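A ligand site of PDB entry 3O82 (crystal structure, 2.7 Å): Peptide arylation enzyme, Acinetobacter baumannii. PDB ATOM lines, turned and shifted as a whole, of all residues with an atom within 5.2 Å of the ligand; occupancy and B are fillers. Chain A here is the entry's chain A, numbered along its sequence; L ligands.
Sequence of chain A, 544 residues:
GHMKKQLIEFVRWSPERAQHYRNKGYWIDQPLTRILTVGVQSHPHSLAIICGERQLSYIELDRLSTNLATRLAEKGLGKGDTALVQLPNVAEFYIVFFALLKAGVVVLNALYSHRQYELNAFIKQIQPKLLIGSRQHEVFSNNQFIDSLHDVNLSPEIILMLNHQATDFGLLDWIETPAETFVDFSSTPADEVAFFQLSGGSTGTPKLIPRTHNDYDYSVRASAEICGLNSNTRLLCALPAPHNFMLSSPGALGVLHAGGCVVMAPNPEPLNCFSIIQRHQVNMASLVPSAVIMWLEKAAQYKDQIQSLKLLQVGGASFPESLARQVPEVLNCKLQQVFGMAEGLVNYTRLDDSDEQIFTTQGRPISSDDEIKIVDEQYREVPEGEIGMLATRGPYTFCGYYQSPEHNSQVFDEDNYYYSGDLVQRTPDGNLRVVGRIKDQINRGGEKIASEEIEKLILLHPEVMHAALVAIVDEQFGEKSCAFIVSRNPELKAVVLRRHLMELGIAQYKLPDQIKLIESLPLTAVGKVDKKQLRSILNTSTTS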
ATOM      1  N   LEU A 198      22.995 -26.019 -12.988  1.00  0.00           N
ATOM      2  CA  LEU A 198      23.607 -25.936 -11.624  1.00  0.00           C
ATOM      3  C   LEU A 198      23.848 -24.524 -11.187  1.00  0.00           C
ATOM      4  O   LEU A 198      24.395 -23.743 -11.969  1.00  0.00           O
ATOM      5  CB  LEU A 198      25.002 -26.546 -11.617  1.00  0.00           C
ATOM      6  CG  LEU A 198      25.284 -27.942 -12.114  1.00  0.00           C
ATOM      7  CD1 LEU A 198      26.740 -28.050 -12.390  1.00  0.00           C
ATOM      8  CD2 LEU A 198      24.867 -28.945 -11.071  1.00  0.00           C
ATOM      9  N   SER A 199      23.540 -24.181  -9.933  1.00  0.00           N
ATOM     10  CA  SER A 199      23.877 -22.840  -9.433  1.00  0.00           C
ATOM     11  C   SER A 199      25.391 -22.640  -9.199  1.00  0.00           C
ATOM     12  O   SER A 199      26.117 -23.535  -8.818  1.00  0.00           O
ATOM     13  CB  SER A 199      23.100 -22.524  -8.180  1.00  0.00           C
ATOM     14  OG  SER A 199      23.367 -23.517  -7.218  1.00  0.00           O
ATOM     15  N   GLY A 200      25.869 -21.430  -9.470  1.00  0.00           N
ATOM     16  CA  GLY A 200      27.217 -21.015  -9.062  1.00  0.00           C
ATOM     17  C   GLY A 200      27.132 -20.245  -7.737  1.00  0.00           C
ATOM     18  O   GLY A 200      28.154 -19.939  -7.105  1.00  0.00           O
ATOM     19  N   GLY A 201      25.884 -19.941  -7.322  1.00  0.00           N
ATOM     20  CA  GLY A 201      25.598 -19.171  -6.091  1.00  0.00           C
ATOM     21  C   GLY A 201      25.714 -19.947  -4.767  1.00  0.00           C
ATOM     22  O   GLY A 201      25.461 -19.393  -3.685  1.00  0.00           O
ATOM     23  N   HIS A 243      27.978 -24.349 -18.845  1.00  0.00           N
ATOM     24  CA  HIS A 243      27.626 -23.176 -18.082  1.00  0.00           C
ATOM     25  C   HIS A 243      26.521 -22.397 -18.777  1.00  0.00           C
ATOM     26  O   HIS A 243      26.597 -22.194 -20.006  1.00  0.00           O
ATOM     27  CB  HIS A 243      28.839 -22.290 -17.913  1.00  0.00           C
ATOM     28  CG  HIS A 243      28.648 -21.248 -16.862  1.00  0.00           C
ATOM     29  ND1 HIS A 243      27.874 -20.130 -17.062  1.00  0.00           N
ATOM     30  CD2 HIS A 243      29.111 -21.170 -15.588  1.00  0.00           C
ATOM     31  CE1 HIS A 243      27.873 -19.394 -15.968  1.00  0.00           C
ATOM     32  NE2 HIS A 243      28.607 -20.012 -15.058  1.00  0.00           N
ATOM     33  N   ASN A 244      25.534 -21.938 -17.997  1.00  0.00           N
ATOM     34  CA  ASN A 244      24.319 -21.354 -18.564  1.00  0.00           C
ATOM     35  C   ASN A 244      24.668 -20.219 -19.553  1.00  0.00           C
ATOM     36  O   ASN A 244      24.210 -20.229 -20.691  1.00  0.00           O
ATOM     37  CB  ASN A 244      23.406 -20.863 -17.444  1.00  0.00           C
ATOM     38  CG  ASN A 244      21.969 -20.588 -17.894  1.00  0.00           C
ATOM     39  OD1 ASN A 244      21.285 -21.437 -18.472  1.00  0.00           O
ATOM     40  ND2 ASN A 244      21.492 -19.400 -17.583  1.00  0.00           N
ATOM     41  N   PHE A 245      25.508 -19.289 -19.129  1.00  0.00           N
ATOM     42  CA  PHE A 245      26.044 -18.240 -19.974  1.00  0.00           C
ATOM     43  C   PHE A 245      26.522 -18.815 -21.316  1.00  0.00           C
ATOM     44  O   PHE A 245      26.147 -18.306 -22.364  1.00  0.00           O
ATOM     45  CB  PHE A 245      27.162 -17.544 -19.199  1.00  0.00           C
ATOM     46  CG  PHE A 245      27.764 -16.345 -19.877  1.00  0.00           C
ATOM     47  CD1 PHE A 245      27.131 -15.693 -20.946  1.00  0.00           C
ATOM     48  CD2 PHE A 245      28.973 -15.833 -19.397  1.00  0.00           C
ATOM     49  CE1 PHE A 245      27.721 -14.564 -21.574  1.00  0.00           C
ATOM     50  CE2 PHE A 245      29.609 -14.714 -19.999  1.00  0.00           C
ATOM     51  CZ  PHE A 245      28.974 -14.067 -21.084  1.00  0.00           C
ATOM     52  N   SER A 249      23.188 -18.053 -23.390  1.00  0.00           N
ATOM     53  CA  SER A 249      23.064 -16.626 -23.196  1.00  0.00           C
ATOM     54  C   SER A 249      23.941 -15.783 -24.100  1.00  0.00           C
ATOM     55  O   SER A 249      24.774 -15.003 -23.636  1.00  0.00           O
ATOM     56  CB  SER A 249      23.276 -16.275 -21.721  1.00  0.00           C
ATOM     57  OG  SER A 249      22.299 -16.923 -20.913  1.00  0.00           O
ATOM     58  N   VAL A 314      30.463  -9.951 -21.818  1.00  0.00           N
ATOM     59  CA  VAL A 314      31.120 -10.213 -20.550  1.00  0.00           C
ATOM     60  C   VAL A 314      30.079 -10.349 -19.483  1.00  0.00           C
ATOM     61  O   VAL A 314      29.268  -9.446 -19.289  1.00  0.00           O
ATOM     62  CB  VAL A 314      32.066  -9.088 -20.142  1.00  0.00           C
ATOM     63  CG1 VAL A 314      32.709  -9.390 -18.803  1.00  0.00           C
ATOM     64  CG2 VAL A 314      33.094  -8.881 -21.193  1.00  0.00           C
ATOM     65  N   GLY A 315      30.103 -11.464 -18.788  1.00  0.00           N
ATOM     66  CA  GLY A 315      29.196 -11.698 -17.681  1.00  0.00           C
ATOM     67  C   GLY A 315      29.834 -12.593 -16.643  1.00  0.00           C
ATOM     68  O   GLY A 315      30.919 -13.147 -16.865  1.00  0.00           O
ATOM     69  N   GLY A 316      29.190 -12.733 -15.502  1.00  0.00           N
ATOM     70  CA  GLY A 316      29.542 -13.778 -14.574  1.00  0.00           C
ATOM     71  C   GLY A 316      30.073 -13.295 -13.243  1.00  0.00           C
ATOM     72  O   GLY A 316      30.124 -14.044 -12.317  1.00  0.00           O
ATOM     73  N   ALA A 317      30.438 -12.033 -13.141  1.00  0.00           N
ATOM     74  CA  ALA A 317      31.085 -11.553 -11.947  1.00  0.00           C
ATOM     75  C   ALA A 317      31.194 -10.076 -12.187  1.00  0.00           C
ATOM     76  O   ALA A 317      30.980  -9.631 -13.322  1.00  0.00           O
ATOM     77  CB  ALA A 317      32.483 -12.199 -11.755  1.00  0.00           C
ATOM     78  N   SER A 318      31.489  -9.328 -11.137  1.00  0.00           N
ATOM     79  CA  SER A 318      31.515  -7.870 -11.195  1.00  0.00           C
ATOM     80  C   SER A 318      32.514  -7.407 -12.241  1.00  0.00           C
ATOM     81  O   SER A 318      33.619  -7.912 -12.305  1.00  0.00           O
ATOM     82  CB  SER A 318      31.859  -7.292  -9.826  1.00  0.00           C
ATOM     83  OG  SER A 318      31.984  -5.876  -9.876  1.00  0.00           O
ATOM     84  N   PHE A 319      32.090  -6.461 -13.074  1.00  0.00           N
ATOM     85  CA  PHE A 319      32.896  -5.976 -14.174  1.00  0.00           C
ATOM     86  C   PHE A 319      33.069  -4.449 -14.108  1.00  0.00           C
ATOM     87  O   PHE A 319      32.238  -3.700 -14.588  1.00  0.00           O
ATOM     88  CB  PHE A 319      32.279  -6.405 -15.532  1.00  0.00           C
ATOM     89  CG  PHE A 319      33.210  -6.294 -16.696  1.00  0.00           C
ATOM     90  CD1 PHE A 319      34.533  -6.748 -16.629  1.00  0.00           C
ATOM     91  CD2 PHE A 319      32.779  -5.767 -17.888  1.00  0.00           C
ATOM     92  CE1 PHE A 319      35.402  -6.633 -17.734  1.00  0.00           C
ATOM     93  CE2 PHE A 319      33.660  -5.664 -19.003  1.00  0.00           C
ATOM     94  CZ  PHE A 319      34.967  -6.088 -18.912  1.00  0.00           C
ATOM     95  N   GLN A 337      27.217  -6.386 -22.138  1.00  0.00           N
ATOM     96  CA  GLN A 337      27.268  -6.890 -20.770  1.00  0.00           C
ATOM     97  C   GLN A 337      26.115  -7.809 -20.421  1.00  0.00           C
ATOM     98  O   GLN A 337      24.958  -7.545 -20.768  1.00  0.00           O
ATOM     99  CB  GLN A 337      27.315  -5.739 -19.811  1.00  0.00           C
ATOM    100  CG  GLN A 337      28.582  -4.954 -19.907  1.00  0.00           C
ATOM    101  CD  GLN A 337      28.955  -4.377 -18.579  1.00  0.00           C
ATOM    102  OE1 GLN A 337      29.086  -5.081 -17.578  1.00  0.00           O
ATOM    103  NE2 GLN A 337      29.088  -3.096 -18.554  1.00  0.00           N
ATOM    104  N   VAL A 338      26.427  -8.907 -19.728  1.00  0.00           N
ATOM    105  CA  VAL A 338      25.435  -9.919 -19.450  1.00  0.00           C
ATOM    106  C   VAL A 338      25.418 -10.234 -17.960  1.00  0.00           C
ATOM    107  O   VAL A 338      26.431 -10.552 -17.403  1.00  0.00           O
ATOM    108  CB  VAL A 338      25.646 -11.178 -20.351  1.00  0.00           C
ATOM    109  CG1 VAL A 338      24.499 -12.113 -20.288  1.00  0.00           C
ATOM    110  CG2 VAL A 338      25.764 -10.745 -21.750  1.00  0.00           C
ATOM    111  N   PHE A 339      24.250 -10.118 -17.343  1.00  0.00           N
ATOM    112  CA  PHE A 339      24.043 -10.515 -15.934  1.00  0.00           C
ATOM    113  C   PHE A 339      22.883 -11.529 -15.867  1.00  0.00           C
ATOM    114  O   PHE A 339      21.704 -11.162 -15.936  1.00  0.00           O
ATOM    115  CB  PHE A 339      23.755  -9.273 -15.063  1.00  0.00           C
ATOM    116  CG  PHE A 339      23.012  -9.545 -13.799  1.00  0.00           C
ATOM    117  CD1 PHE A 339      23.384 -10.562 -12.939  1.00  0.00           C
ATOM    118  CD2 PHE A 339      21.921  -8.766 -13.447  1.00  0.00           C
ATOM    119  CE1 PHE A 339      22.657 -10.782 -11.739  1.00  0.00           C
ATOM    120  CE2 PHE A 339      21.206  -8.992 -12.265  1.00  0.00           C
ATOM    121  CZ  PHE A 339      21.586  -9.981 -11.410  1.00  0.00           C
ATOM    122  N   GLY A 340      23.250 -12.794 -15.726  1.00  0.00           N
ATOM    123  CA  GLY A 340      22.297 -13.864 -15.781  1.00  0.00           C
ATOM    124  C   GLY A 340      22.559 -14.754 -14.618  1.00  0.00           C
ATOM    125  O   GLY A 340      23.504 -14.547 -13.878  1.00  0.00           O
ATOM    126  N   MET A 341      21.684 -15.734 -14.439  1.00  0.00           N
ATOM    127  CA  MET A 341      21.865 -16.720 -13.390  1.00  0.00           C
ATOM    128  C   MET A 341      21.319 -18.061 -13.933  1.00  0.00           C
ATOM    129  O   MET A 341      20.335 -18.109 -14.638  1.00  0.00           O
ATOM    130  CB  MET A 341      21.150 -16.276 -12.122  1.00  0.00           C
ATOM    131  CG  MET A 341      19.736 -15.801 -12.377  1.00  0.00           C
ATOM    132  SD  MET A 341      18.947 -15.121 -10.916  1.00  0.00           S
ATOM    133  CE  MET A 341      19.623 -13.448 -11.013  1.00  0.00           C
ATOM    134  N   ALA A 342      22.003 -19.156 -13.632  1.00  0.00           N
ATOM    135  CA  ALA A 342      21.524 -20.481 -13.983  1.00  0.00           C
ATOM    136  C   ALA A 342      20.026 -20.660 -13.641  1.00  0.00           C
ATOM    137  O   ALA A 342      19.295 -21.435 -14.284  1.00  0.00           O
ATOM    138  CB  ALA A 342      22.402 -21.566 -13.294  1.00  0.00           C
ATOM    139  N   GLU A 343      19.560 -19.920 -12.639  1.00  0.00           N
ATOM    140  CA  GLU A 343      18.221 -20.108 -12.144  1.00  0.00           C
ATOM    141  C   GLU A 343      17.188 -19.581 -13.094  1.00  0.00           C
ATOM    142  O   GLU A 343      16.027 -19.883 -12.974  1.00  0.00           O
ATOM    143  CB  GLU A 343      18.048 -19.383 -10.806  1.00  0.00           C
ATOM    144  CG  GLU A 343      18.524 -20.180  -9.606  1.00  0.00           C
ATOM    145  CD  GLU A 343      19.993 -19.994  -9.328  1.00  0.00           C
ATOM    146  OE1 GLU A 343      20.704 -19.445 -10.185  1.00  0.00           O
ATOM    147  OE2 GLU A 343      20.447 -20.400  -8.236  1.00  0.00           O
ATOM    148  N   VAL A 346      18.035 -13.479 -17.239  1.00  0.00           N
ATOM    149  CA  VAL A 346      19.218 -13.000 -17.878  1.00  0.00           C
ATOM    150  C   VAL A 346      18.933 -11.606 -18.355  1.00  0.00           C
ATOM    151  O   VAL A 346      17.850 -11.374 -18.907  1.00  0.00           O
ATOM    152  CB  VAL A 346      19.663 -13.846 -19.106  1.00  0.00           C
ATOM    153  CG1 VAL A 346      20.924 -13.269 -19.656  1.00  0.00           C
ATOM    154  CG2 VAL A 346      19.884 -15.315 -18.729  1.00  0.00           C
ATOM    155  N   GLN A 362      24.486  -3.468 -16.337  1.00  0.00           N
ATOM    156  CA  GLN A 362      24.432  -4.832 -16.792  1.00  0.00           C
ATOM    157  C   GLN A 362      23.113  -5.108 -17.511  1.00  0.00           C
ATOM    158  O   GLN A 362      22.567  -6.183 -17.383  1.00  0.00           O
ATOM    159  CB  GLN A 362      24.650  -5.800 -15.644  1.00  0.00           C
ATOM    160  CG  GLN A 362      26.077  -5.947 -15.186  1.00  0.00           C
ATOM    161  CD  GLN A 362      26.626  -4.653 -14.640  1.00  0.00           C
ATOM    162  OE1 GLN A 362      26.049  -4.054 -13.733  1.00  0.00           O
ATOM    163  NE2 GLN A 362      27.733  -4.203 -15.195  1.00  0.00           N
ATOM    164  N   SER A 420      17.808 -14.093  -5.611  1.00  0.00           N
ATOM    165  CA  SER A 420      19.173 -14.511  -5.946  1.00  0.00           C
ATOM    166  C   SER A 420      20.211 -14.141  -4.907  1.00  0.00           C
ATOM    167  O   SER A 420      21.244 -14.787  -4.806  1.00  0.00           O
ATOM    168  CB  SER A 420      19.607 -13.925  -7.285  1.00  0.00           C
ATOM    169  OG  SER A 420      19.782 -12.520  -7.185  1.00  0.00           O
ATOM    170  N   ASP A 422      21.406 -10.992  -5.044  1.00  0.00           N
ATOM    171  CA  ASP A 422      22.160  -9.934  -5.690  1.00  0.00           C
ATOM    172  C   ASP A 422      21.641  -8.622  -5.246  1.00  0.00           C
ATOM    173  O   ASP A 422      20.432  -8.464  -5.018  1.00  0.00           O
ATOM    174  CB  ASP A 422      22.053 -10.061  -7.196  1.00  0.00           C
ATOM    175  CG  ASP A 422      22.804 -11.234  -7.696  1.00  0.00           C
ATOM    176  OD1 ASP A 422      22.230 -12.049  -8.421  1.00  0.00           O
ATOM    177  OD2 ASP A 422      23.955 -11.376  -7.308  1.00  0.00           O
ATOM    178  N   VAL A 434      24.488  -4.244 -11.174  1.00  0.00           N
ATOM    179  CA  VAL A 434      24.832  -5.209 -10.098  1.00  0.00           C
ATOM    180  C   VAL A 434      25.874  -4.571  -9.223  1.00  0.00           C
ATOM    181  O   VAL A 434      26.982  -4.244  -9.706  1.00  0.00           O
ATOM    182  CB  VAL A 434      25.441  -6.550 -10.597  1.00  0.00           C
ATOM    183  CG1 VAL A 434      25.584  -7.500  -9.479  1.00  0.00           C
ATOM    184  CG2 VAL A 434      24.554  -7.188 -11.586  1.00  0.00           C
HETATM  185  S1  LIG L   1      25.638 -18.404 -12.499  1.00  0.00           S
HETATM  186  N1  LIG L   1      27.917  -8.711 -12.997  1.00  0.00           N
HETATM  187  C1  LIG L   1      27.989  -9.043 -11.714  1.00  0.00           C
HETATM  188  N2  LIG L   1      27.624 -10.263 -11.262  1.00  0.00           N
HETATM  189  C2  LIG L   1      27.157 -11.214 -12.109  1.00  0.00           C
HETATM  190  C3  LIG L   1      27.045 -10.896 -13.460  1.00  0.00           C
HETATM  191  C4  LIG L   1      27.433  -9.614 -13.882  1.00  0.00           C
HETATM  192  N3  LIG L   1      27.343  -9.234 -15.164  1.00  0.00           N
HETATM  193  N4  LIG L   1      26.560 -12.009 -14.052  1.00  0.00           N
HETATM  194  C5  LIG L   1      26.348 -12.986 -13.134  1.00  0.00           C
HETATM  195  N5  LIG L   1      26.745 -12.509 -11.932  1.00  0.00           N
HETATM  196  O1  LIG L   1      26.914 -16.304 -13.744  1.00  0.00           O
HETATM  197  C6  LIG L   1      26.651 -13.250 -10.638  1.00  0.00           C
HETATM  198  C7  LIG L   1      25.559 -16.165 -15.687  1.00  0.00           C
HETATM  199  C8  LIG L   1      25.301 -12.881 -10.029  1.00  0.00           C
HETATM  200  O2  LIG L   1      25.433 -12.836  -8.649  1.00  0.00           O
HETATM  201  C9  LIG L   1      25.978 -16.779 -14.384  1.00  0.00           C
HETATM  202  C10 LIG L   1      24.536 -16.712 -16.435  1.00  0.00           C
HETATM  203  O3  LIG L   1      23.834 -17.825 -16.034  1.00  0.00           O
HETATM  204  C11 LIG L   1      24.378 -14.056 -10.315  1.00  0.00           C
HETATM  205  O4  LIG L   1      23.468 -14.312  -9.261  1.00  0.00           O
HETATM  206  C12 LIG L   1      24.222 -16.131 -17.635  1.00  0.00           C
HETATM  207  O5  LIG L   1      23.221 -16.652 -18.353  1.00  0.00           O
HETATM  208  C13 LIG L   1      25.345 -15.209 -10.433  1.00  0.00           C
HETATM  209  O6  LIG L   1      26.546 -14.646 -10.900  1.00  0.00           O
HETATM  210  C14 LIG L   1      24.875 -15.048 -18.154  1.00  0.00           C
HETATM  211  C15 LIG L   1      24.860 -16.174 -11.439  1.00  0.00           C
HETATM  212  O7  LIG L   1      25.755 -17.283 -11.443  1.00  0.00           O
HETATM  213  C16 LIG L   1      25.896 -14.518 -17.406  1.00  0.00           C
HETATM  214  C17 LIG L   1      26.251 -15.086 -16.175  1.00  0.00           C
HETATM  215  N6  LIG L   1      25.317 -17.825 -13.937  1.00  0.00           N
HETATM  216  O8  LIG L   1      24.437 -19.053 -12.084  1.00  0.00           O
HETATM  217  O9  LIG L   1      26.816 -19.198 -12.596  1.00  0.00           O
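O of Ala 317 sits close to N1 of the ligand, 3.2 Å away. Residues that only touch the ligand: Gly 200 (3.8 Å), Phe 245 (3.5 Å), Gly 315 (3.98 Å), Ser 318 (3.6 Å), Phe 339 (3.5 Å), Gly 340 (3.2 Å), Val 346 (3.6 Å), Gln 362 (3.5 Å) and Val 434 (3.6 Å). Hydrophobic or aromatic side chains that line the ligand: His 243, Phe 245, Val 338, Phe 339, Met 341, Ala 342, Val 346 and Val 434. 18 residues have an atom within 4 Å of the ligand: Gly 200, His 243, Asn 244, Phe 245, Ser 249, Gly 315, Gly 316, Ala 317, Ser 318, Val 338, Phe 339, Gly 340, Met 341, Ala 342, Val 346, Gln 362, Asp 422 and Val 434. Along chain A the residues within 4 Å of the ligand span positions 200 to 434.
An oxygen (O8) of the ligand lies within hydrogen-bond range of the backbone NH (N) of Ala 342. O3 of the ligand sits close to N of Met 341 (3.4 Å). A nitrogen (N4) of the ligand lies within hydrogen-bond range of the backbone NH (N) of Gly 316. O2 of the ligand is in hydrogen-bond range of OD2 of Asp 422 (2.5 Å). The backbone carbonyl oxygen (O) of Val 338 sits at hydrogen-bond distance from a nitrogen (N3) of the ligand (2.8 Å). The side-chain hydroxyl of Ser 249 sits at hydrogen-bond distance from an oxygen (O5) of the ligand, at 2.7 Å. The side-chain amide nitrogen of Asn 244 is in hydrogen-bond range of an oxygen (O3) of the ligand, 3.2 Å away. O9 of the ligand sits at hydrogen-bond distance from NE2 of His 243, 3.2 Å away.
N of Phe 245 lies within hydrogen-bond range of ND1 of His 243 (3.3 Å). The side-chain amide nitrogen of Gln 362 sits at hydrogen-bond distance from the side-chain amide oxygen of Gln 337, 2.9 Å away. The side-chain carboxylate (OD1) of Asp 422 sits at hydrogen-bond distance from the side-chain hydroxyl (OG) of Ser 420. O of Val 314 sits at hydrogen-bond distance from N of Val 338, at 2.9 Å. OE1 of Gln 362 lies within hydrogen-bond range of N of Val 434, at 3.0 Å. ND2 of Asn 244 lies within hydrogen-bond range of O of Met 341, at 3.4 Å.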
